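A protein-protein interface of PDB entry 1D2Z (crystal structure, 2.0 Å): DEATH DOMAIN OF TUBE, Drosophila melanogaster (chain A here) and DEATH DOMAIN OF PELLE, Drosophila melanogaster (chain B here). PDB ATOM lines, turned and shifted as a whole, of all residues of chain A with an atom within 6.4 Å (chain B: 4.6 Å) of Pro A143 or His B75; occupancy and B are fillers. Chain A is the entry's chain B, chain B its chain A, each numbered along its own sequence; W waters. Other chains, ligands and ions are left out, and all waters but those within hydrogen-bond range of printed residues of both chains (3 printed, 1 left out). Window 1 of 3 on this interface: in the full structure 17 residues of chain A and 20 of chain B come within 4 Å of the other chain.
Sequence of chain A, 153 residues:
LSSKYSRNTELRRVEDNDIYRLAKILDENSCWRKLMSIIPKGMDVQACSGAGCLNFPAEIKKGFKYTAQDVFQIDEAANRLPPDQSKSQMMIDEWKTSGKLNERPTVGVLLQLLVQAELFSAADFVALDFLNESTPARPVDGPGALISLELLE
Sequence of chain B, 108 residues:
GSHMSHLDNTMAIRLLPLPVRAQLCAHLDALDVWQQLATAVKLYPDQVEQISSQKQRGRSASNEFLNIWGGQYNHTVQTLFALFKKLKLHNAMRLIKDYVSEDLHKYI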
ATOM      1  N   GLU A 118       9.990  28.435   3.254  1.00  0.00           N
ATOM      2  CA  GLU A 118      11.217  27.780   2.792  1.00  0.00           C
ATOM      3  C   GLU A 118      11.946  28.516   1.666  1.00  0.00           C
ATOM      4  O   GLU A 118      12.602  27.894   0.822  1.00  0.00           O
ATOM      5  CB  GLU A 118      10.955  26.320   2.396  1.00  0.00           C
ATOM      6  CG  GLU A 118      10.387  25.478   3.538  1.00  0.00           C
ATOM      7  CD  GLU A 118      10.459  23.975   3.291  1.00  0.00           C
ATOM      8  OE1 GLU A 118      10.306  23.524   2.133  1.00  0.00           O
ATOM      9  OE2 GLU A 118      10.659  23.238   4.272  1.00  0.00           O
ATOM     10  N   SER A 121      16.956  31.169   0.009  1.00  0.00           N
ATOM     11  CA  SER A 121      17.881  32.063  -0.684  1.00  0.00           C
ATOM     12  C   SER A 121      17.609  33.494  -0.229  1.00  0.00           C
ATOM     13  O   SER A 121      18.532  34.264   0.044  1.00  0.00           O
ATOM     14  CB  SER A 121      17.698  31.966  -2.193  1.00  0.00           C
ATOM     15  OG  SER A 121      18.785  31.291  -2.780  1.00  0.00           O
ATOM     16  N   ARG A 138      17.975  24.852   8.728  1.00  0.00           N
ATOM     17  CA  ARG A 138      17.205  24.142   7.718  1.00  0.00           C
ATOM     18  C   ARG A 138      16.419  22.989   8.338  1.00  0.00           C
ATOM     19  O   ARG A 138      16.774  22.489   9.407  1.00  0.00           O
ATOM     20  CB  ARG A 138      18.149  23.564   6.656  1.00  0.00           C
ATOM     21  CG  ARG A 138      19.017  24.592   5.953  1.00  0.00           C
ATOM     22  CD  ARG A 138      18.153  25.639   5.287  1.00  0.00           C
ATOM     23  NE  ARG A 138      18.943  26.576   4.503  1.00  0.00           N
ATOM     24  CZ  ARG A 138      19.204  26.433   3.209  1.00  0.00           C
ATOM     25  NH1 ARG A 138      18.734  25.380   2.540  1.00  0.00           N
ATOM     26  NH2 ARG A 138      19.927  27.356   2.581  1.00  0.00           N
ATOM     27  N   ASP A 141      13.932  17.289   6.785  1.00  0.00           N
ATOM     28  CA  ASP A 141      13.393  16.659   5.588  1.00  0.00           C
ATOM     29  C   ASP A 141      12.889  17.696   4.594  1.00  0.00           C
ATOM     30  O   ASP A 141      12.678  18.864   4.942  1.00  0.00           O
ATOM     31  CB  ASP A 141      12.243  15.708   5.952  1.00  0.00           C
ATOM     32  CG  ASP A 141      12.698  14.523   6.794  1.00  0.00           C
ATOM     33  OD1 ASP A 141      13.630  13.803   6.368  1.00  0.00           O
ATOM     34  OD2 ASP A 141      12.111  14.302   7.878  1.00  0.00           O
ATOM     35  N   GLY A 142      12.679  17.253   3.359  1.00  0.00           N
ATOM     36  CA  GLY A 142      12.184  18.141   2.328  1.00  0.00           C
ATOM     37  C   GLY A 142      13.264  18.775   1.471  1.00  0.00           C
ATOM     38  O   GLY A 142      14.458  18.597   1.721  1.00  0.00           O
ATOM     39  N   PRO A 143      12.857  19.573   0.472  1.00  0.00           N
ATOM     40  CA  PRO A 143      13.730  20.277  -0.475  1.00  0.00           C
ATOM     41  C   PRO A 143      14.703  21.290   0.130  1.00  0.00           C
ATOM     42  O   PRO A 143      15.722  21.602  -0.479  1.00  0.00           O
ATOM     43  CB  PRO A 143      12.736  20.922  -1.437  1.00  0.00           C
ATOM     44  CG  PRO A 143      11.515  21.150  -0.567  1.00  0.00           C
ATOM     45  CD  PRO A 143      11.437  19.869   0.202  1.00  0.00           C
ATOM     46  N   GLY A 144      14.410  21.780   1.334  1.00  0.00           N
ATOM     47  CA  GLY A 144      15.297  22.743   1.967  1.00  0.00           C
ATOM     48  C   GLY A 144      16.360  22.137   2.869  1.00  0.00           C
ATOM     49  O   GLY A 144      17.264  22.836   3.331  1.00  0.00           O
ATOM     50  N   ALA A 145      16.275  20.832   3.096  1.00  0.00           N
ATOM     51  CA  ALA A 145      17.219  20.138   3.967  1.00  0.00           C
ATOM     52  C   ALA A 145      18.558  19.822   3.315  1.00  0.00           C
ATOM     53  O   ALA A 145      18.648  19.608   2.103  1.00  0.00           O
ATOM     54  CB  ALA A 145      16.595  18.852   4.489  1.00  0.00           C
ATOM     55  N   LEU A 146      19.586  19.762   4.151  1.00  0.00           N
ATOM     56  CA  LEU A 146      20.935  19.439   3.712  1.00  0.00           C
ATOM     57  C   LEU A 146      21.022  17.922   3.571  1.00  0.00           C
ATOM     58  O   LEU A 146      20.160  17.188   4.071  1.00  0.00           O
ATOM     59  CB  LEU A 146      21.951  19.930   4.745  1.00  0.00           C
ATOM     60  CG  LEU A 146      21.799  21.390   5.183  1.00  0.00           C
ATOM     61  CD1 LEU A 146      22.849  21.735   6.230  1.00  0.00           C
ATOM     62  CD2 LEU A 146      21.905  22.316   3.977  1.00  0.00           C
ATOM     63  N   ILE A 147      22.041  17.456   2.859  1.00  0.00           N
ATOM     64  CA  ILE A 147      22.243  16.026   2.651  1.00  0.00           C
ATOM     65  C   ILE A 147      23.647  15.666   3.131  1.00  0.00           C
ATOM     66  O   ILE A 147      24.628  16.306   2.748  1.00  0.00           O
ATOM     67  CB  ILE A 147      22.081  15.650   1.156  1.00  0.00           C
ATOM     68  CG1 ILE A 147      20.724  16.142   0.639  1.00  0.00           C
ATOM     69  CG2 ILE A 147      22.190  14.139   0.975  1.00  0.00           C
ATOM     70  CD1 ILE A 147      20.486  15.891  -0.830  1.00  0.00           C
ATOM     71  N   ALA B  12      27.473  28.355  -4.020  1.00  0.00           N
ATOM     72  CA  ALA B  12      26.064  28.049  -4.200  1.00  0.00           C
ATOM     73  C   ALA B  12      25.904  27.481  -5.606  1.00  0.00           C
ATOM     74  O   ALA B  12      26.600  27.906  -6.534  1.00  0.00           O
ATOM     75  CB  ALA B  12      25.235  29.317  -4.050  1.00  0.00           C
ATOM     76  N   ILE B  13      25.005  26.507  -5.751  1.00  0.00           N
ATOM     77  CA  ILE B  13      24.719  25.878  -7.038  1.00  0.00           C
ATOM     78  C   ILE B  13      24.414  26.927  -8.109  1.00  0.00           C
ATOM     79  O   ILE B  13      24.827  26.787  -9.265  1.00  0.00           O
ATOM     80  CB  ILE B  13      23.506  24.909  -6.909  1.00  0.00           C
ATOM     81  CG1 ILE B  13      23.908  23.684  -6.077  1.00  0.00           C
ATOM     82  CG2 ILE B  13      22.960  24.533  -8.289  1.00  0.00           C
ATOM     83  CD1 ILE B  13      22.749  22.797  -5.657  1.00  0.00           C
ATOM     84  N   VAL B  41      14.759  14.712  -3.295  1.00  0.00           N
ATOM     85  CA  VAL B  41      14.770  15.901  -2.438  1.00  0.00           C
ATOM     86  C   VAL B  41      13.343  16.312  -2.070  1.00  0.00           C
ATOM     87  O   VAL B  41      13.122  17.335  -1.428  1.00  0.00           O
ATOM     88  CB  VAL B  41      15.506  17.091  -3.106  1.00  0.00           C
ATOM     89  CG1 VAL B  41      16.929  16.689  -3.464  1.00  0.00           C
ATOM     90  CG2 VAL B  41      14.753  17.561  -4.333  1.00  0.00           C
ATOM     91  N   LYS B  42      12.379  15.513  -2.515  1.00  0.00           N
ATOM     92  CA  LYS B  42      10.968  15.742  -2.233  1.00  0.00           C
ATOM     93  C   LYS B  42      10.407  17.072  -2.727  1.00  0.00           C
ATOM     94  O   LYS B  42       9.748  17.789  -1.972  1.00  0.00           O
ATOM     95  CB  LYS B  42      10.693  15.581  -0.728  1.00  0.00           C
ATOM     96  CG  LYS B  42      11.064  14.216  -0.175  1.00  0.00           C
ATOM     97  CD  LYS B  42      10.793  14.128   1.322  1.00  0.00           C
ATOM     98  CE  LYS B  42      11.247  12.781   1.882  1.00  0.00           C
ATOM     99  NZ  LYS B  42      11.042  12.677   3.359  1.00  0.00           N
ATOM    100  N   LEU B  43      10.676  17.413  -3.985  1.00  0.00           N
ATOM    101  CA  LEU B  43      10.135  18.644  -4.558  1.00  0.00           C
ATOM    102  C   LEU B  43       8.614  18.493  -4.581  1.00  0.00           C
ATOM    103  O   LEU B  43       8.098  17.374  -4.693  1.00  0.00           O
ATOM    104  CB  LEU B  43      10.640  18.866  -5.992  1.00  0.00           C
ATOM    105  CG  LEU B  43      12.093  19.303  -6.212  1.00  0.00           C
ATOM    106  CD1 LEU B  43      12.284  19.704  -7.680  1.00  0.00           C
ATOM    107  CD2 LEU B  43      12.419  20.481  -5.315  1.00  0.00           C
ATOM    108  N   TYR B  44       7.909  19.614  -4.482  1.00  0.00           N
ATOM    109  CA  TYR B  44       6.452  19.610  -4.481  1.00  0.00           C
ATOM    110  C   TYR B  44       5.879  19.436  -5.889  1.00  0.00           C
ATOM    111  O   TYR B  44       6.576  19.663  -6.887  1.00  0.00           O
ATOM    112  CB  TYR B  44       5.916  20.878  -3.808  1.00  0.00           C
ATOM    113  CG  TYR B  44       6.102  20.874  -2.304  1.00  0.00           C
ATOM    114  CD1 TYR B  44       7.276  21.365  -1.726  1.00  0.00           C
ATOM    115  CD2 TYR B  44       5.115  20.358  -1.458  1.00  0.00           C
ATOM    116  CE1 TYR B  44       7.466  21.341  -0.350  1.00  0.00           C
ATOM    117  CE2 TYR B  44       5.297  20.329  -0.069  1.00  0.00           C
ATOM    118  CZ  TYR B  44       6.474  20.821   0.474  1.00  0.00           C
ATOM    119  OH  TYR B  44       6.672  20.787   1.838  1.00  0.00           O
ATOM    120  N   TRP B  69      15.766  23.717  -7.075  1.00  0.00           N
ATOM    121  CA  TRP B  69      16.436  23.253  -5.863  1.00  0.00           C
ATOM    122  C   TRP B  69      17.608  24.148  -5.442  1.00  0.00           C
ATOM    123  O   TRP B  69      17.755  24.473  -4.264  1.00  0.00           O
ATOM    124  CB  TRP B  69      16.884  21.803  -6.060  1.00  0.00           C
ATOM    125  CG  TRP B  69      17.282  21.099  -4.807  1.00  0.00           C
ATOM    126  CD1 TRP B  69      16.510  20.894  -3.688  1.00  0.00           C
ATOM    127  CD2 TRP B  69      18.548  20.494  -4.537  1.00  0.00           C
ATOM    128  NE1 TRP B  69      17.223  20.202  -2.742  1.00  0.00           N
ATOM    129  CE2 TRP B  69      18.477  19.940  -3.234  1.00  0.00           C
ATOM    130  CE3 TRP B  69      19.739  20.363  -5.266  1.00  0.00           C
ATOM    131  CZ2 TRP B  69      19.551  19.267  -2.652  1.00  0.00           C
ATOM    132  CZ3 TRP B  69      20.808  19.693  -4.683  1.00  0.00           C
ATOM    133  CH2 TRP B  69      20.707  19.155  -3.389  1.00  0.00           C
ATOM    134  N   GLY B  70      18.418  24.574  -6.405  1.00  0.00           N
ATOM    135  CA  GLY B  70      19.542  25.435  -6.081  1.00  0.00           C
ATOM    136  C   GLY B  70      19.114  26.878  -5.886  1.00  0.00           C
ATOM    137  O   GLY B  70      19.551  27.548  -4.955  1.00  0.00           O
ATOM    138  N   TYR B  73      16.217  27.172  -2.630  1.00  0.00           N
ATOM    139  CA  TYR B  73      16.780  26.677  -1.372  1.00  0.00           C
ATOM    140  C   TYR B  73      18.235  27.024  -1.103  1.00  0.00           C
ATOM    141  O   TYR B  73      18.784  26.642  -0.072  1.00  0.00           O
ATOM    142  CB  TYR B  73      16.527  25.177  -1.248  1.00  0.00           C
ATOM    143  CG  TYR B  73      15.077  24.834  -1.505  1.00  0.00           C
ATOM    144  CD1 TYR B  73      14.123  24.960  -0.495  1.00  0.00           C
ATOM    145  CD2 TYR B  73      14.648  24.441  -2.769  1.00  0.00           C
ATOM    146  CE1 TYR B  73      12.784  24.707  -0.736  1.00  0.00           C
ATOM    147  CE2 TYR B  73      13.302  24.187  -3.028  1.00  0.00           C
ATOM    148  CZ  TYR B  73      12.377  24.321  -1.999  1.00  0.00           C
ATOM    149  OH  TYR B  73      11.057  24.051  -2.224  1.00  0.00           O
ATOM    150  N   ASN B  74      18.855  27.748  -2.031  1.00  0.00           N
ATOM    151  CA  ASN B  74      20.239  28.198  -1.873  1.00  0.00           C
ATOM    152  C   ASN B  74      21.207  27.072  -1.501  1.00  0.00           C
ATOM    153  O   ASN B  74      22.041  27.235  -0.615  1.00  0.00           O
ATOM    154  CB  ASN B  74      20.284  29.314  -0.812  1.00  0.00           C
ATOM    155  CG  ASN B  74      21.526  30.190  -0.919  1.00  0.00           C
ATOM    156  OD1 ASN B  74      22.128  30.309  -1.989  1.00  0.00           O
ATOM    157  ND2 ASN B  74      21.908  30.815   0.196  1.00  0.00           N
ATOM    158  N   HIS B  75      21.074  25.919  -2.152  1.00  0.00           N
ATOM    159  CA  HIS B  75      21.953  24.788  -1.868  1.00  0.00           C
ATOM    160  C   HIS B  75      23.326  24.954  -2.514  1.00  0.00           C
ATOM    161  O   HIS B  75      23.465  25.635  -3.534  1.00  0.00           O
ATOM    162  CB  HIS B  75      21.306  23.468  -2.289  1.00  0.00           C
ATOM    163  CG  HIS B  75      20.221  23.013  -1.365  1.00  0.00           C
ATOM    164  ND1 HIS B  75      20.414  22.876  -0.009  1.00  0.00           N
ATOM    165  CD2 HIS B  75      18.932  22.673  -1.598  1.00  0.00           C
ATOM    166  CE1 HIS B  75      19.290  22.467   0.556  1.00  0.00           C
ATOM    167  NE2 HIS B  75      18.374  22.335  -0.387  1.00  0.00           N
ATOM    168  N   THR B  76      24.328  24.359  -1.876  1.00  0.00           N
ATOM    169  CA  THR B  76      25.721  24.418  -2.321  1.00  0.00           C
ATOM    170  C   THR B  76      26.111  23.252  -3.224  1.00  0.00           C
ATOM    171  O   THR B  76      25.408  22.234  -3.296  1.00  0.00           O
ATOM    172  CB  THR B  76      26.687  24.390  -1.118  1.00  0.00           C
ATOM    173  OG1 THR B  76      26.613  23.108  -0.483  1.00  0.00           O
ATOM    174  CG2 THR B  76      26.344  25.487  -0.108  1.00  0.00           C
ATOM    175  N   VAL B  77      27.257  23.396  -3.890  1.00  0.00           N
ATOM    176  CA  VAL B  77      27.747  22.355  -4.778  1.00  0.00           C
ATOM    177  C   VAL B  77      28.042  21.096  -3.962  1.00  0.00           C
ATOM    178  O   VAL B  77      27.839  19.983  -4.442  1.00  0.00           O
ATOM    179  CB  VAL B  77      29.017  22.806  -5.549  1.00  0.00           C
ATOM    180  CG1 VAL B  77      29.505  21.697  -6.451  1.00  0.00           C
ATOM    181  CG2 VAL B  77      28.710  24.029  -6.391  1.00  0.00           C
ATOM    182  N   THR B  79      26.394  20.012  -1.362  1.00  0.00           N
ATOM    183  CA  THR B  79      25.117  19.348  -1.114  1.00  0.00           C
ATOM    184  C   THR B  79      24.658  18.624  -2.382  1.00  0.00           C
ATOM    185  O   THR B  79      24.116  17.524  -2.310  1.00  0.00           O
ATOM    186  CB  THR B  79      24.056  20.350  -0.602  1.00  0.00           C
ATOM    187  OG1 THR B  79      24.527  20.925   0.624  1.00  0.00           O
ATOM    188  CG2 THR B  79      22.722  19.653  -0.327  1.00  0.00           C
HETATM  189  O   HOH W   1       9.353  24.259  -0.283  1.00  0.00           O
HETATM  190  O   HOH W   2      24.438  18.880   2.524  1.00  0.00           O
HETATM  191  O   HOH W   3       9.143  21.060   2.913  1.00  0.00           O
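Water W2 bridges the backbone carbonyl oxygen of Ile A147 and the side-chain hydroxyl of Thr B79.
Water W1 lies within hydrogen-bond range of OH of Tyr B73 (2.6 Å) and OE1 of Glu A118 (2.7 Å).
Water W3 lies within hydrogen-bond range of OH of Tyr B44 and OE1 of Glu A118.
NE2 of His B75 sits close to NE1 of Trp B69 (3.4 Å).
The side-chain hydroxyl (OG1) of Thr B76 sits at hydrogen-bond distance from the side-chain hydroxyl (OG1) of Thr B79 (3.2 Å).
The backbone NH of Ile B13 lies within hydrogen-bond range of the backbone carbonyl oxygen of His B75 (2.8 Å).
NH1 of Arg A138 lies within hydrogen-bond range of O of Gly A144, 3.0 Å away.
NE1 of Trp B69 lies within hydrogen-bond range of O of Pro A143.
The guanidinium group (NH1) of Arg A138 lies within hydrogen-bond range of the backbone carbonyl oxygen (O) of Tyr B73, at 2.9 Å.
N of Pro A143 lies close to O of Val B41, 2.9 Å away.
A ring nitrogen (NE2) of His B75 lies within hydrogen-bond range of the backbone carbonyl oxygen (O) of Pro A143 (2.8 Å).
Of the 10 printed residues of chain A, 8 touch a printed residue of chain B.
Among the printed residues, 17 pairs touch across the chains.
Of the printed residues of chain B, Arg A138 touches Tyr B73, Asn B74 and His B75.
Asp A141 touches none of the printed residues of chain B.
Of the printed residues of chain B, Ala A145 touches His B75.
Ala B12 touches none of the printed residues of chain A.
Printed residues of chain A within 4 Å of Val B41: Gly A142 (3.2 Å) and Pro A143 (2.9 Å).
Of the printed residues of chain A, Tyr B73 touches Glu A118 (3.6 Å), Arg A138 (2.9 Å), Pro A143 (3.4 Å) and Gly A144 (3.5 Å).
His B75 touches just these residues of chain A: Arg A138 (3.6 Å), Pro A143 (2.8 Å), Gly A144 (3.5 Å) and Ala A145 (3.3 Å).
The nearest residue of chain A that does not touch His B75 is Leu A146 (4.3 Å).
Among the printed residues, pairs that only touch across the chains: Ser A121 with Asn B74, Gly A142 with Val B41, Ala A145 with His B75, Pro A143 with Tyr B73, Pro A143 with Lys B42, Gly A144 with His B75, Gly A144 with Tyr B73, Glu A118 with Tyr B73, Arg A138 with His B75, Arg A138 with Asn B74, Pro A143 with Leu B43, Ile A147 with Thr B79 and Ile A147 with Trp B69.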
